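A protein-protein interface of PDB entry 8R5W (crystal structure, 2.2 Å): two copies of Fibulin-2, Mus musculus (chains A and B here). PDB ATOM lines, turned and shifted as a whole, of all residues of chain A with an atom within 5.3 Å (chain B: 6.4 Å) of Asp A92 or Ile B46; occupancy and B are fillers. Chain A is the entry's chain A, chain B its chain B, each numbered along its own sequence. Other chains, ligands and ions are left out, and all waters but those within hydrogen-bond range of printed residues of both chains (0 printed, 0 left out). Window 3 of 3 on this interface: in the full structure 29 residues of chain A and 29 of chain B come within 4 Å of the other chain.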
ATOM      1  N   CYS A  74       9.798   8.446  25.365  1.00  0.00           N
ATOM      2  CA  CYS A  74       9.421   9.631  24.611  1.00  0.00           C
ATOM      3  C   CYS A  74      10.650  10.439  24.184  1.00  0.00           C
ATOM      4  O   CYS A  74      10.563  11.210  23.235  1.00  0.00           O
ATOM      5  CB  CYS A  74       8.426  10.473  25.401  1.00  0.00           C
ATOM      6  SG  CYS A  74       6.930   9.564  25.887  1.00  0.00           S
ATOM      7  N   GLY A  75      11.801  10.230  24.848  1.00  0.00           N
ATOM      8  CA  GLY A  75      12.945  11.131  24.719  1.00  0.00           C
ATOM      9  C   GLY A  75      13.175  11.990  25.968  1.00  0.00           C
ATOM     10  O   GLY A  75      12.303  12.092  26.817  1.00  0.00           O
ATOM     11  N   TYR A  87       6.788  14.322  18.252  1.00  0.00           N
ATOM     12  CA  TYR A  87       6.830  12.964  18.741  1.00  0.00           C
ATOM     13  C   TYR A  87       6.892  13.006  20.277  1.00  0.00           C
ATOM     14  O   TYR A  87       6.041  12.400  20.947  1.00  0.00           O
ATOM     15  CB  TYR A  87       7.986  12.138  18.168  1.00  0.00           C
ATOM     16  CG  TYR A  87       8.027  10.712  18.689  1.00  0.00           C
ATOM     17  CD1 TYR A  87       7.222   9.706  18.178  1.00  0.00           C
ATOM     18  CD2 TYR A  87       8.858  10.403  19.748  1.00  0.00           C
ATOM     19  CE1 TYR A  87       7.233   8.434  18.728  1.00  0.00           C
ATOM     20  CE2 TYR A  87       8.931   9.110  20.260  1.00  0.00           C
ATOM     21  CZ  TYR A  87       8.109   8.124  19.754  1.00  0.00           C
ATOM     22  OH  TYR A  87       8.149   6.889  20.331  1.00  0.00           O
ATOM     23  N   LYS A  88       7.885  13.736  20.799  1.00  0.00           N
ATOM     24  CA  LYS A  88       8.150  13.781  22.221  1.00  0.00           C
ATOM     25  C   LYS A  88       6.976  14.388  22.992  1.00  0.00           C
ATOM     26  O   LYS A  88       6.504  13.848  23.999  1.00  0.00           O
ATOM     27  CB  LYS A  88       9.446  14.545  22.511  1.00  0.00           C
ATOM     28  CG  LYS A  88       9.799  14.656  23.990  1.00  0.00           C
ATOM     29  CD  LYS A  88      11.281  14.877  24.298  1.00  0.00           C
ATOM     30  CE  LYS A  88      11.652  16.300  24.529  1.00  0.00           C
ATOM     31  NZ  LYS A  88      11.143  17.136  23.439  1.00  0.00           N
ATOM     32  N   GLN A  89       6.505  15.530  22.496  1.00  0.00           N
ATOM     33  CA  GLN A  89       5.421  16.251  23.125  1.00  0.00           C
ATOM     34  C   GLN A  89       4.201  15.348  23.238  1.00  0.00           C
ATOM     35  O   GLN A  89       3.623  15.237  24.307  1.00  0.00           O
ATOM     36  CB  GLN A  89       5.100  17.493  22.302  1.00  0.00           C
ATOM     37  CG  GLN A  89       3.902  18.292  22.804  1.00  0.00           C
ATOM     38  CD  GLN A  89       3.718  19.561  21.998  1.00  0.00           C
ATOM     39  OE1 GLN A  89       3.411  19.521  20.803  1.00  0.00           O
ATOM     40  NE2 GLN A  89       4.040  20.682  22.618  1.00  0.00           N
ATOM     41  N   CYS A  90       3.801  14.709  22.134  1.00  0.00           N
ATOM     42  CA  CYS A  90       2.581  13.935  22.126  1.00  0.00           C
ATOM     43  C   CYS A  90       2.753  12.646  22.930  1.00  0.00           C
ATOM     44  O   CYS A  90       1.830  12.212  23.599  1.00  0.00           O
ATOM     45  CB  CYS A  90       2.098  13.739  20.700  1.00  0.00           C
ATOM     46  SG  CYS A  90       1.464  15.279  20.002  1.00  0.00           S
ATOM     47  N   CYS A  91       3.955  12.081  22.923  1.00  0.00           N
ATOM     48  CA  CYS A  91       4.240  10.928  23.759  1.00  0.00           C
ATOM     49  C   CYS A  91       4.113  11.291  25.250  1.00  0.00           C
ATOM     50  O   CYS A  91       3.422  10.601  26.017  1.00  0.00           O
ATOM     51  CB  CYS A  91       5.604  10.404  23.376  1.00  0.00           C
ATOM     52  SG  CYS A  91       6.063   8.877  24.204  1.00  0.00           S
ATOM     53  N   ASP A  92       4.738  12.402  25.652  1.00  0.00           N
ATOM     54  CA  ASP A  92       4.663  12.870  27.031  1.00  0.00           C
ATOM     55  C   ASP A  92       3.205  13.162  27.437  1.00  0.00           C
ATOM     56  O   ASP A  92       2.769  12.784  28.515  1.00  0.00           O
ATOM     57  CB  ASP A  92       5.518  14.109  27.242  1.00  0.00           C
ATOM     58  CG  ASP A  92       7.022  13.887  27.258  1.00  0.00           C
ATOM     59  OD1 ASP A  92       7.444  12.721  27.481  1.00  0.00           O
ATOM     60  OD2 ASP A  92       7.774  14.870  27.013  1.00  0.00           O
ATOM     61  N   CYS A  93       2.473  13.893  26.593  1.00  0.00           N
ATOM     62  CA  CYS A  93       1.121  14.317  26.917  1.00  0.00           C
ATOM     63  C   CYS A  93       0.166  13.128  26.966  1.00  0.00           C
ATOM     64  O   CYS A  93      -0.754  13.097  27.766  1.00  0.00           O
ATOM     65  CB  CYS A  93       0.599  15.354  25.937  1.00  0.00           C
ATOM     66  SG  CYS A  93       1.551  16.887  25.972  1.00  0.00           S
ATOM     67  N   CYS A  94       0.365  12.166  26.068  1.00  0.00           N
ATOM     68  CA  CYS A  94      -0.393  10.935  26.133  1.00  0.00           C
ATOM     69  C   CYS A  94      -0.116  10.260  27.468  1.00  0.00           C
ATOM     70  O   CYS A  94      -1.052   9.838  28.139  1.00  0.00           O
ATOM     71  CB  CYS A  94      -0.088  10.011  24.961  1.00  0.00           C
ATOM     72  SG  CYS A  94      -1.036   8.467  25.027  1.00  0.00           S
ATOM     73  N   GLY A  95       1.171  10.204  27.853  1.00  0.00           N
ATOM     74  CA  GLY A  95       1.599   9.581  29.098  1.00  0.00           C
ATOM     75  C   GLY A  95       0.902  10.180  30.326  1.00  0.00           C
ATOM     76  O   GLY A  95       0.564   9.463  31.258  1.00  0.00           O
ATOM     77  N   LEU A  96       0.651  11.492  30.306  1.00  0.00           N
ATOM     78  CA  LEU A  96      -0.098  12.138  31.372  1.00  0.00           C
ATOM     79  C   LEU A  96      -1.479  11.494  31.505  1.00  0.00           C
ATOM     80  O   LEU A  96      -1.917  11.204  32.603  1.00  0.00           O
ATOM     81  CB  LEU A  96      -0.245  13.643  31.166  1.00  0.00           C
ATOM     82  CG  LEU A  96       1.037  14.475  31.217  1.00  0.00           C
ATOM     83  CD1 LEU A  96       0.702  15.948  31.001  1.00  0.00           C
ATOM     84  CD2 LEU A  96       1.836  14.292  32.480  1.00  0.00           C
ATOM     85  N   SER B  41       9.350  14.420  39.477  1.00  0.00           N
ATOM     86  CA  SER B  41       8.751  13.344  38.691  1.00  0.00           C
ATOM     87  C   SER B  41       8.586  13.745  37.225  1.00  0.00           C
ATOM     88  O   SER B  41       8.545  14.919  36.902  1.00  0.00           O
ATOM     89  CB  SER B  41       7.458  12.871  39.301  1.00  0.00           C
ATOM     90  OG  SER B  41       6.353  13.622  38.854  1.00  0.00           O
ATOM     91  N   ASP B  42       8.528  12.744  36.341  1.00  0.00           N
ATOM     92  CA  ASP B  42       8.294  12.917  34.915  1.00  0.00           C
ATOM     93  C   ASP B  42       6.982  13.674  34.684  1.00  0.00           C
ATOM     94  O   ASP B  42       6.933  14.601  33.869  1.00  0.00           O
ATOM     95  CB  ASP B  42       8.319  11.568  34.202  1.00  0.00           C
ATOM     96  CG  ASP B  42       8.526  11.577  32.693  1.00  0.00           C
ATOM     97  OD1 ASP B  42       8.909  12.660  32.164  1.00  0.00           O
ATOM     98  OD2 ASP B  42       8.271  10.508  32.066  1.00  0.00           O
ATOM     99  N   ILE B  43       5.936  13.258  35.414  1.00  0.00           N
ATOM    100  CA  ILE B  43       4.615  13.851  35.301  1.00  0.00           C
ATOM    101  C   ILE B  43       4.705  15.357  35.527  1.00  0.00           C
ATOM    102  O   ILE B  43       4.140  16.131  34.768  1.00  0.00           O
ATOM    103  CB  ILE B  43       3.654  13.181  36.300  1.00  0.00           C
ATOM    104  CG1 ILE B  43       3.427  11.700  35.965  1.00  0.00           C
ATOM    105  CG2 ILE B  43       2.332  13.937  36.416  1.00  0.00           C
ATOM    106  CD1 ILE B  43       2.826  11.452  34.593  1.00  0.00           C
ATOM    107  N   CYS B  44       5.408  15.743  36.595  1.00  0.00           N
ATOM    108  CA  CYS B  44       5.572  17.130  36.967  1.00  0.00           C
ATOM    109  C   CYS B  44       6.369  17.891  35.911  1.00  0.00           C
ATOM    110  O   CYS B  44       5.981  18.985  35.522  1.00  0.00           O
ATOM    111  CB  CYS B  44       6.250  17.252  38.337  1.00  0.00           C
ATOM    112  SG  CYS B  44       6.277  18.956  38.978  1.00  0.00           S
ATOM    113  N   ARG B  45       7.481  17.316  35.458  1.00  0.00           N
ATOM    114  CA  ARG B  45       8.346  18.003  34.504  1.00  0.00           C
ATOM    115  C   ARG B  45       7.610  18.232  33.178  1.00  0.00           C
ATOM    116  O   ARG B  45       7.745  19.298  32.566  1.00  0.00           O
ATOM    117  CB  ARG B  45       9.663  17.248  34.318  1.00  0.00           C
ATOM    118  CG  ARG B  45       9.628  16.030  33.411  1.00  0.00           C
ATOM    119  CD  ARG B  45      10.941  15.327  33.314  1.00  0.00           C
ATOM    120  NE  ARG B  45      11.313  14.803  34.635  1.00  0.00           N
ATOM    121  CZ  ARG B  45      12.530  14.398  34.957  1.00  0.00           C
ATOM    122  NH1 ARG B  45      13.515  14.359  34.064  1.00  0.00           N
ATOM    123  NH2 ARG B  45      12.781  14.000  36.195  1.00  0.00           N
ATOM    124  N   ILE B  46       6.816  17.236  32.758  1.00  0.00           N
ATOM    125  CA  ILE B  46       6.067  17.335  31.512  1.00  0.00           C
ATOM    126  C   ILE B  46       5.041  18.463  31.639  1.00  0.00           C
ATOM    127  O   ILE B  46       4.951  19.297  30.751  1.00  0.00           O
ATOM    128  CB  ILE B  46       5.382  16.004  31.139  1.00  0.00           C
ATOM    129  CG1 ILE B  46       6.370  14.928  30.716  1.00  0.00           C
ATOM    130  CG2 ILE B  46       4.311  16.222  30.074  1.00  0.00           C
ATOM    131  CD1 ILE B  46       5.823  13.511  30.849  1.00  0.00           C
ATOM    132  N   ALA B  47       4.263  18.468  32.735  1.00  0.00           N
ATOM    133  CA  ALA B  47       3.219  19.456  32.930  1.00  0.00           C
ATOM    134  C   ALA B  47       3.793  20.873  33.028  1.00  0.00           C
ATOM    135  O   ALA B  47       3.208  21.815  32.507  1.00  0.00           O
ATOM    136  CB  ALA B  47       2.423  19.091  34.144  1.00  0.00           C
ATOM    137  N   GLN B  48       4.929  21.013  33.707  1.00  0.00           N
ATOM    138  CA  GLN B  48       5.583  22.302  33.859  1.00  0.00           C
ATOM    139  C   GLN B  48       5.958  22.864  32.486  1.00  0.00           C
ATOM    140  O   GLN B  48       5.602  24.002  32.134  1.00  0.00           O
ATOM    141  CB  GLN B  48       6.864  22.183  34.683  1.00  0.00           C
ATOM    142  CG  GLN B  48       6.991  23.319  35.686  1.00  0.00           C
ATOM    143  CD  GLN B  48       8.118  23.143  36.675  1.00  0.00           C
ATOM    144  OE1 GLN B  48       8.177  22.142  37.385  1.00  0.00           O
ATOM    145  NE2 GLN B  48       8.985  24.137  36.747  1.00  0.00           N
ATOM    146  N   ARG B  49       6.696  22.044  31.728  1.00  0.00           N
ATOM    147  CA  ARG B  49       7.200  22.447  30.430  1.00  0.00           C
ATOM    148  C   ARG B  49       6.033  22.781  29.500  1.00  0.00           C
ATOM    149  O   ARG B  49       6.053  23.799  28.818  1.00  0.00           O
ATOM    150  CB  ARG B  49       8.105  21.338  29.878  1.00  0.00           C
ATOM    151  CG  ARG B  49       8.699  21.651  28.515  1.00  0.00           C
ATOM    152  CD  ARG B  49       9.444  20.484  27.945  1.00  0.00           C
ATOM    153  NE  ARG B  49       8.446  19.460  27.629  1.00  0.00           N
ATOM    154  CZ  ARG B  49       8.418  18.216  28.084  1.00  0.00           C
ATOM    155  NH1 ARG B  49       9.304  17.775  28.966  1.00  0.00           N
ATOM    156  NH2 ARG B  49       7.495  17.379  27.629  1.00  0.00           N
ATOM    157  N   GLN B  50       5.020  21.902  29.474  1.00  0.00           N
ATOM    158  CA  GLN B  50       3.936  22.062  28.529  1.00  0.00           C
ATOM    159  C   GLN B  50       3.147  23.335  28.829  1.00  0.00           C
ATOM    160  O   GLN B  50       2.732  24.026  27.905  1.00  0.00           O
ATOM    161  CB  GLN B  50       2.992  20.856  28.515  1.00  0.00           C
ATOM    162  CG  GLN B  50       3.567  19.629  27.826  1.00  0.00           C
ATOM    163  CD  GLN B  50       3.955  19.917  26.394  1.00  0.00           C
ATOM    164  OE1 GLN B  50       3.227  20.576  25.646  1.00  0.00           O
ATOM    165  NE2 GLN B  50       5.130  19.446  26.015  1.00  0.00           N
ATOM    166  N   CYS B  51       2.891  23.621  30.112  1.00  0.00           N
ATOM    167  CA  CYS B  51       2.113  24.798  30.471  1.00  0.00           C
ATOM    168  C   CYS B  51       2.944  26.066  30.280  1.00  0.00           C
ATOM    169  O   CYS B  51       2.396  27.119  29.950  1.00  0.00           O
ATOM    170  CB  CYS B  51       1.531  24.670  31.859  1.00  0.00           C
ATOM    171  SG  CYS B  51       0.356  23.301  31.963  1.00  0.00           S
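The side-chain amide nitrogen of Gln A89 sits at hydrogen-bond distance from the side-chain amide oxygen of Gln B50.
OD2 of Asp A92 is in salt-bridge range of NH2 of Arg B49, 2.6 Å away.
The side-chain sulfur (SG) of Cys A74 lies within hydrogen-bond range of the backbone NH (N) of Asp A92, at 3.6 Å.
The side-chain hydroxyl (OG) of Ser B41 sits close to the backbone NH (N) of Ile B43 (3.5 Å).
The side-chain sulfur (SG) of Cys A74 forms a disulfide with the side-chain sulfur (SG) of Cys A91, 2.0 Å away.
Among the printed residues, pairs that only touch across the chains: Asp A92 with Ile B46, Cys A93 with Gln B50, Leu A96 with Ile B43 and Leu A96 with Ile B46.
Of the printed residues of chain B, Gln A89 touches Gln B50.
Of the printed residues of chain B, Asp A92 touches Ile B46 (3.7 Å) and Arg B49 (2.6 Å).
Printed residues of chain B within 4 Å of Cys A93: Gln B50.
Of the printed residues of chain B, Leu A96 touches Ile B43 and Ile B46.
Ile B46 touches just these residues of chain A: Asp A92 and Leu A96.
Printed residues of chain A within 4 Å of Arg B49: Asp A92.
The nearest printed residue of chain B that does not touch Cys A93 is Ile B46 (4.6 Å).
Printed residues of chain B that touch a printed residue of chain A: Ile B43, Ile B46, Arg B49 and Gln B50.
Printed residues of chain A that touch a printed residue of chain B: Gln A89, Asp A92, Cys A93 and Leu A96.
Hydrophobic or aromatic side chains of chain A that line the printed part of chain B: Leu A96.
Among the printed residues, Asp or Glu carboxylates within 4 Å of a Lys or Arg side-chain nitrogen of the other chain: Asp A92 with Arg B49.
No position is printed for both chains.
Of the 6 pairs that touch across the chains among the printed residues, none has its exchanged pair printed and touching as well.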
